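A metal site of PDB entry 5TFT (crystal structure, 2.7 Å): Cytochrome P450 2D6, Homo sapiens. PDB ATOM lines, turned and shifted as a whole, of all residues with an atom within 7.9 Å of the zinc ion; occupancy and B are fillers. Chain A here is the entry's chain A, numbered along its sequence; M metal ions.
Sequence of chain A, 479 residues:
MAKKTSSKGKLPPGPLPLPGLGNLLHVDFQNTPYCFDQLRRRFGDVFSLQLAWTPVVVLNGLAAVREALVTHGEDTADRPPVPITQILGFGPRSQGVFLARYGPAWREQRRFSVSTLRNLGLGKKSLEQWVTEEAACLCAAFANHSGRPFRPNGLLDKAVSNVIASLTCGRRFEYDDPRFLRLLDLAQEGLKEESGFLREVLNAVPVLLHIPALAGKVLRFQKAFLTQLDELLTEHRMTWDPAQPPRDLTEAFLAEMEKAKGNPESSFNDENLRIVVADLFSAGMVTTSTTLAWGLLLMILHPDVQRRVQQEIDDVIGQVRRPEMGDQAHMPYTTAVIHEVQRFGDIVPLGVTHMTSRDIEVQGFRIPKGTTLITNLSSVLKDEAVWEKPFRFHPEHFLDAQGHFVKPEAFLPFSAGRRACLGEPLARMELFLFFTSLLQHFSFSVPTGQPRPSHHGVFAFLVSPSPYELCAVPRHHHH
The zinc ion is bound by NE2 of His 236 (2.0 Å), OE2 of Glu 251 (2.0 Å) and OD2 of Asp 248 (2.0 Å).
O of Cys 169 sits close to NE2 of His 236, 3.5 Å away. The side-chain hydroxyl of Thr 239 sits at hydrogen-bond distance from the backbone carbonyl oxygen of His 236. The backbone NH (N) of Arg 247 lies within hydrogen-bond range of the side-chain carboxylate (OE1) of Glu 251, at 3.0 Å. OD2 of Asp 248 lies close to N of Gly 170 (3.2 Å). The side-chain carboxylate of Asp 248 sits close to the backbone NH of Thr 250. SG of Cys 169 lies within hydrogen-bond range of OG1 of Thr 168 (3.8 Å).
Merely in contact with the zinc ion: Cys 169. Within 4 Å of the zinc ion: Cys 169, His 236, Asp 248 and Glu 251. The nearest printed residue that does not touch the zinc ion is Arg 247 (4.2 Å).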
ATOM      1  N   TRP A 130       9.964  19.563 -22.002  1.00  0.00           N
ATOM      2  CA  TRP A 130      11.126  20.264 -21.450  1.00  0.00           C
ATOM      3  C   TRP A 130      11.547  21.439 -22.329  1.00  0.00           C
ATOM      4  O   TRP A 130      12.026  22.450 -21.819  1.00  0.00           O
ATOM      5  CB  TRP A 130      12.308  19.306 -21.272  1.00  0.00           C
ATOM      6  CG  TRP A 130      12.255  18.498 -20.006  1.00  0.00           C
ATOM      7  CD1 TRP A 130      12.033  18.968 -18.749  1.00  0.00           C
ATOM      8  CD2 TRP A 130      12.458  17.086 -19.885  1.00  0.00           C
ATOM      9  NE1 TRP A 130      12.070  17.921 -17.847  1.00  0.00           N
ATOM     10  CE2 TRP A 130      12.321  16.757 -18.521  1.00  0.00           C
ATOM     11  CE3 TRP A 130      12.725  16.057 -20.796  1.00  0.00           C
ATOM     12  CZ2 TRP A 130      12.455  15.456 -18.040  1.00  0.00           C
ATOM     13  CZ3 TRP A 130      12.851  14.763 -20.325  1.00  0.00           C
ATOM     14  CH2 TRP A 130      12.725  14.476 -18.959  1.00  0.00           C
ATOM     15  N   ALA A 165      20.470  18.979 -20.556  1.00  0.00           N
ATOM     16  CA  ALA A 165      20.491  18.533 -19.168  1.00  0.00           C
ATOM     17  C   ALA A 165      19.185  17.838 -18.808  1.00  0.00           C
ATOM     18  O   ALA A 165      19.168  16.947 -17.959  1.00  0.00           O
ATOM     19  CB  ALA A 165      20.745  19.709 -18.238  1.00  0.00           C
ATOM     20  N   SER A 166      18.108  18.243 -19.454  1.00  0.00           N
ATOM     21  CA  SER A 166      16.801  17.630 -19.246  1.00  0.00           C
ATOM     22  C   SER A 166      16.765  16.222 -19.824  1.00  0.00           C
ATOM     23  O   SER A 166      16.010  15.372 -19.359  1.00  0.00           O
ATOM     24  CB  SER A 166      15.694  18.483 -19.864  1.00  0.00           C
ATOM     25  OG  SER A 166      15.675  19.779 -19.285  1.00  0.00           O
ATOM     26  N   LEU A 167      17.577  15.981 -20.842  1.00  0.00           N
ATOM     27  CA  LEU A 167      17.622  14.669 -21.472  1.00  0.00           C
ATOM     28  C   LEU A 167      18.683  13.782 -20.845  1.00  0.00           C
ATOM     29  O   LEU A 167      18.497  12.567 -20.706  1.00  0.00           O
ATOM     30  CB  LEU A 167      17.852  14.793 -22.978  1.00  0.00           C
ATOM     31  CG  LEU A 167      16.667  15.418 -23.731  1.00  0.00           C
ATOM     32  CD1 LEU A 167      16.847  15.304 -25.229  1.00  0.00           C
ATOM     33  CD2 LEU A 167      15.351  14.768 -23.302  1.00  0.00           C
ATOM     34  N   THR A 168      19.811  14.374 -20.456  1.00  0.00           N
ATOM     35  CA  THR A 168      20.862  13.623 -19.785  1.00  0.00           C
ATOM     36  C   THR A 168      20.516  13.352 -18.319  1.00  0.00           C
ATOM     37  O   THR A 168      20.374  12.192 -17.922  1.00  0.00           O
ATOM     38  CB  THR A 168      22.211  14.352 -19.850  1.00  0.00           C
ATOM     39  OG1 THR A 168      22.110  15.617 -19.184  1.00  0.00           O
ATOM     40  CG2 THR A 168      22.631  14.565 -21.290  1.00  0.00           C
ATOM     41  N   CYS A 169      20.349  14.403 -17.525  1.00  0.00           N
ATOM     42  CA  CYS A 169      20.190  14.240 -16.078  1.00  0.00           C
ATOM     43  C   CYS A 169      18.772  14.550 -15.559  1.00  0.00           C
ATOM     44  O   CYS A 169      18.547  14.573 -14.354  1.00  0.00           O
ATOM     45  CB  CYS A 169      21.199  15.120 -15.328  1.00  0.00           C
ATOM     46  SG  CYS A 169      22.928  14.707 -15.612  1.00  0.00           S
ATOM     47  N   GLY A 170      17.839  14.782 -16.472  1.00  0.00           N
ATOM     48  CA  GLY A 170      16.443  15.003 -16.091  1.00  0.00           C
ATOM     49  C   GLY A 170      16.197  16.235 -15.232  1.00  0.00           C
ATOM     50  O   GLY A 170      15.333  16.227 -14.363  1.00  0.00           O
ATOM     51  N   ARG A 171      16.953  17.296 -15.490  1.00  0.00           N
ATOM     52  CA  ARG A 171      16.801  18.530 -14.727  1.00  0.00           C
ATOM     53  C   ARG A 171      17.176  19.757 -15.557  1.00  0.00           C
ATOM     54  O   ARG A 171      17.792  19.634 -16.611  1.00  0.00           O
ATOM     55  CB  ARG A 171      17.657  18.508 -13.460  1.00  0.00           C
ATOM     56  CG  ARG A 171      19.128  18.768 -13.745  1.00  0.00           C
ATOM     57  CD  ARG A 171      19.898  19.095 -12.480  1.00  0.00           C
ATOM     58  NE  ARG A 171      19.461  20.355 -11.876  1.00  0.00           N
ATOM     59  CZ  ARG A 171      19.998  20.890 -10.789  1.00  0.00           C
ATOM     60  NH1 ARG A 171      20.994  20.267 -10.169  1.00  0.00           N
ATOM     61  NH2 ARG A 171      19.535  22.034 -10.308  1.00  0.00           N
ATOM     62  N   HIS A 236      23.333  12.993  -9.315  1.00  0.00           N
ATOM     63  CA  HIS A 236      22.234  12.357 -10.027  1.00  0.00           C
ATOM     64  C   HIS A 236      22.122  10.868  -9.714  1.00  0.00           C
ATOM     65  O   HIS A 236      21.029  10.306  -9.715  1.00  0.00           O
ATOM     66  CB  HIS A 236      22.392  12.562 -11.535  1.00  0.00           C
ATOM     67  CG  HIS A 236      21.248  12.017 -12.332  1.00  0.00           C
ATOM     68  ND1 HIS A 236      21.421  11.386 -13.547  1.00  0.00           N
ATOM     69  CD2 HIS A 236      19.916  12.020 -12.102  1.00  0.00           C
ATOM     70  CE1 HIS A 236      20.251  11.021 -14.017  1.00  0.00           C
ATOM     71  NE2 HIS A 236      19.317  11.396 -13.168  1.00  0.00           N
ATOM     72  N   ARG A 237      23.260  10.239  -9.442  1.00  0.00           N
ATOM     73  CA  ARG A 237      23.283   8.817  -9.118  1.00  0.00           C
ATOM     74  C   ARG A 237      22.589   8.568  -7.778  1.00  0.00           C
ATOM     75  O   ARG A 237      22.014   7.508  -7.560  1.00  0.00           O
ATOM     76  CB  ARG A 237      24.719   8.301  -9.082  1.00  0.00           C
ATOM     77  CG  ARG A 237      24.832   6.777  -9.046  1.00  0.00           C
ATOM     78  CD  ARG A 237      26.279   6.334  -8.875  1.00  0.00           C
ATOM     79  NE  ARG A 237      27.140   6.776  -9.968  1.00  0.00           N
ATOM     80  CZ  ARG A 237      27.485   6.017 -11.005  1.00  0.00           C
ATOM     81  NH1 ARG A 237      27.052   4.769 -11.084  1.00  0.00           N
ATOM     82  NH2 ARG A 237      28.277   6.508 -11.944  1.00  0.00           N
ATOM     83  N   THR A 239      19.950  10.328  -6.517  1.00  0.00           N
ATOM     84  CA  THR A 239      18.507  10.518  -6.588  1.00  0.00           C
ATOM     85  C   THR A 239      17.807   9.532  -7.525  1.00  0.00           C
ATOM     86  O   THR A 239      16.581   9.496  -7.601  1.00  0.00           O
ATOM     87  CB  THR A 239      18.159  11.947  -7.045  1.00  0.00           C
ATOM     88  OG1 THR A 239      18.743  12.193  -8.338  1.00  0.00           O
ATOM     89  CG2 THR A 239      18.675  12.975  -6.056  1.00  0.00           C
ATOM     90  N   TRP A 240      18.602   8.719  -8.232  1.00  0.00           N
ATOM     91  CA  TRP A 240      18.055   7.749  -9.188  1.00  0.00           C
ATOM     92  C   TRP A 240      17.243   6.651  -8.494  1.00  0.00           C
ATOM     93  O   TRP A 240      17.726   6.024  -7.547  1.00  0.00           O
ATOM     94  CB  TRP A 240      19.192   7.121 -10.001  1.00  0.00           C
ATOM     95  CG  TRP A 240      18.761   5.966 -10.839  1.00  0.00           C
ATOM     96  CD1 TRP A 240      17.646   5.888 -11.628  1.00  0.00           C
ATOM     97  CD2 TRP A 240      19.428   4.704 -10.977  1.00  0.00           C
ATOM     98  NE1 TRP A 240      17.586   4.663 -12.250  1.00  0.00           N
ATOM     99  CE2 TRP A 240      18.665   3.919 -11.867  1.00  0.00           C
ATOM    100  CE3 TRP A 240      20.601   4.165 -10.445  1.00  0.00           C
ATOM    101  CZ2 TRP A 240      19.034   2.625 -12.225  1.00  0.00           C
ATOM    102  CZ3 TRP A 240      20.967   2.879 -10.796  1.00  0.00           C
ATOM    103  CH2 TRP A 240      20.192   2.123 -11.676  1.00  0.00           C
ATOM    104  N   ASP A 241      16.029   6.428  -8.983  1.00  0.00           N
ATOM    105  CA  ASP A 241      15.167   5.370  -8.455  1.00  0.00           C
ATOM    106  C   ASP A 241      15.012   4.238  -9.467  1.00  0.00           C
ATOM    107  O   ASP A 241      14.235   4.351 -10.415  1.00  0.00           O
ATOM    108  CB  ASP A 241      13.790   5.945  -8.081  1.00  0.00           C
ATOM    109  CG  ASP A 241      12.904   4.928  -7.376  1.00  0.00           C
ATOM    110  OD1 ASP A 241      11.671   5.137  -7.314  1.00  0.00           O
ATOM    111  OD2 ASP A 241      13.433   3.913  -6.869  1.00  0.00           O
ATOM    112  N   PRO A 246      13.243   4.774 -16.408  1.00  0.00           N
ATOM    113  CA  PRO A 246      14.208   5.875 -16.496  1.00  0.00           C
ATOM    114  C   PRO A 246      13.581   7.214 -16.905  1.00  0.00           C
ATOM    115  O   PRO A 246      12.858   7.281 -17.894  1.00  0.00           O
ATOM    116  CB  PRO A 246      15.188   5.394 -17.564  1.00  0.00           C
ATOM    117  CG  PRO A 246      15.116   3.898 -17.475  1.00  0.00           C
ATOM    118  CD  PRO A 246      13.682   3.595 -17.177  1.00  0.00           C
ATOM    119  N   ARG A 247      13.854   8.258 -16.142  1.00  0.00           N
ATOM    120  CA  ARG A 247      13.374   9.602 -16.453  1.00  0.00           C
ATOM    121  C   ARG A 247      14.222  10.278 -17.521  1.00  0.00           C
ATOM    122  O   ARG A 247      13.766  11.195 -18.203  1.00  0.00           O
ATOM    123  CB  ARG A 247      13.363  10.476 -15.203  1.00  0.00           C
ATOM    124  CG  ARG A 247      12.338  10.109 -14.150  1.00  0.00           C
ATOM    125  CD  ARG A 247      12.204  11.222 -13.125  1.00  0.00           C
ATOM    126  NE  ARG A 247      11.686  12.454 -13.718  1.00  0.00           N
ATOM    127  CZ  ARG A 247      12.424  13.498 -14.085  1.00  0.00           C
ATOM    128  NH1 ARG A 247      13.739  13.476 -13.934  1.00  0.00           N
ATOM    129  NH2 ARG A 247      11.838  14.571 -14.612  1.00  0.00           N
ATOM    130  N   ASP A 248      15.469   9.827 -17.645  1.00  0.00           N
ATOM    131  CA  ASP A 248      16.426  10.477 -18.529  1.00  0.00           C
ATOM    132  C   ASP A 248      17.448   9.470 -19.075  1.00  0.00           C
ATOM    133  O   ASP A 248      17.421   8.298 -18.709  1.00  0.00           O
ATOM    134  CB  ASP A 248      17.121  11.621 -17.799  1.00  0.00           C
ATOM    135  CG  ASP A 248      17.620  11.216 -16.424  1.00  0.00           C
ATOM    136  OD1 ASP A 248      18.431  10.281 -16.335  1.00  0.00           O
ATOM    137  OD2 ASP A 248      17.190  11.834 -15.424  1.00  0.00           O
ATOM    138  N   LEU A 249      18.339   9.938 -19.930  1.00  0.00           N
ATOM    139  CA  LEU A 249      19.293   9.064 -20.613  1.00  0.00           C
ATOM    140  C   LEU A 249      20.291   8.450 -19.637  1.00  0.00           C
ATOM    141  O   LEU A 249      20.680   7.288 -19.785  1.00  0.00           O
ATOM    142  CB  LEU A 249      20.025   9.828 -21.707  1.00  0.00           C
ATOM    143  CG  LEU A 249      21.065   9.054 -22.523  1.00  0.00           C
ATOM    144  CD1 LEU A 249      20.912   9.368 -24.000  1.00  0.00           C
ATOM    145  CD2 LEU A 249      22.479   9.370 -22.063  1.00  0.00           C
ATOM    146  N   THR A 250      20.708   9.234 -18.649  1.00  0.00           N
ATOM    147  CA  THR A 250      21.673   8.763 -17.658  1.00  0.00           C
ATOM    148  C   THR A 250      21.101   7.597 -16.864  1.00  0.00           C
ATOM    149  O   THR A 250      21.798   6.599 -16.615  1.00  0.00           O
ATOM    150  CB  THR A 250      22.098   9.892 -16.702  1.00  0.00           C
ATOM    151  OG1 THR A 250      22.666  10.981 -17.457  1.00  0.00           O
ATOM    152  CG2 THR A 250      23.124   9.405 -15.706  1.00  0.00           C
ATOM    153  N   GLU A 251      19.841   7.709 -16.458  1.00  0.00           N
ATOM    154  CA  GLU A 251      19.173   6.637 -15.720  1.00  0.00           C
ATOM    155  C   GLU A 251      19.041   5.387 -16.579  1.00  0.00           C
ATOM    156  O   GLU A 251      19.232   4.269 -16.101  1.00  0.00           O
ATOM    157  CB  GLU A 251      17.799   7.094 -15.229  1.00  0.00           C
ATOM    158  CG  GLU A 251      17.858   8.167 -14.149  1.00  0.00           C
ATOM    159  CD  GLU A 251      16.490   8.574 -13.647  1.00  0.00           C
ATOM    160  OE1 GLU A 251      15.545   7.765 -13.770  1.00  0.00           O
ATOM    161  OE2 GLU A 251      16.359   9.703 -13.127  1.00  0.00           O
ATOM    162  N   ALA A 252      18.715   5.592 -17.848  1.00  0.00           N
ATOM    163  CA  ALA A 252      18.627   4.494 -18.802  1.00  0.00           C
ATOM    164  C   ALA A 252      20.007   3.854 -18.995  1.00  0.00           C
ATOM    165  O   ALA A 252      20.121   2.635 -19.176  1.00  0.00           O
ATOM    166  CB  ALA A 252      18.085   4.987 -20.134  1.00  0.00           C
ATOM    167  N   LEU A 254      22.408   3.933 -16.640  1.00  0.00           N
ATOM    168  CA  LEU A 254      22.681   3.271 -15.365  1.00  0.00           C
ATOM    169  C   LEU A 254      21.997   1.913 -15.290  1.00  0.00           C
ATOM    170  O   LEU A 254      22.577   0.946 -14.805  1.00  0.00           O
ATOM    171  CB  LEU A 254      22.231   4.149 -14.188  1.00  0.00           C
ATOM    172  CG  LEU A 254      23.037   5.426 -13.925  1.00  0.00           C
ATOM    173  CD1 LEU A 254      22.351   6.294 -12.896  1.00  0.00           C
ATOM    174  CD2 LEU A 254      24.465   5.097 -13.490  1.00  0.00           C
HETATM  175 ZN    ZN M   1      17.385  11.347 -13.497  1.00  0.00          ZN
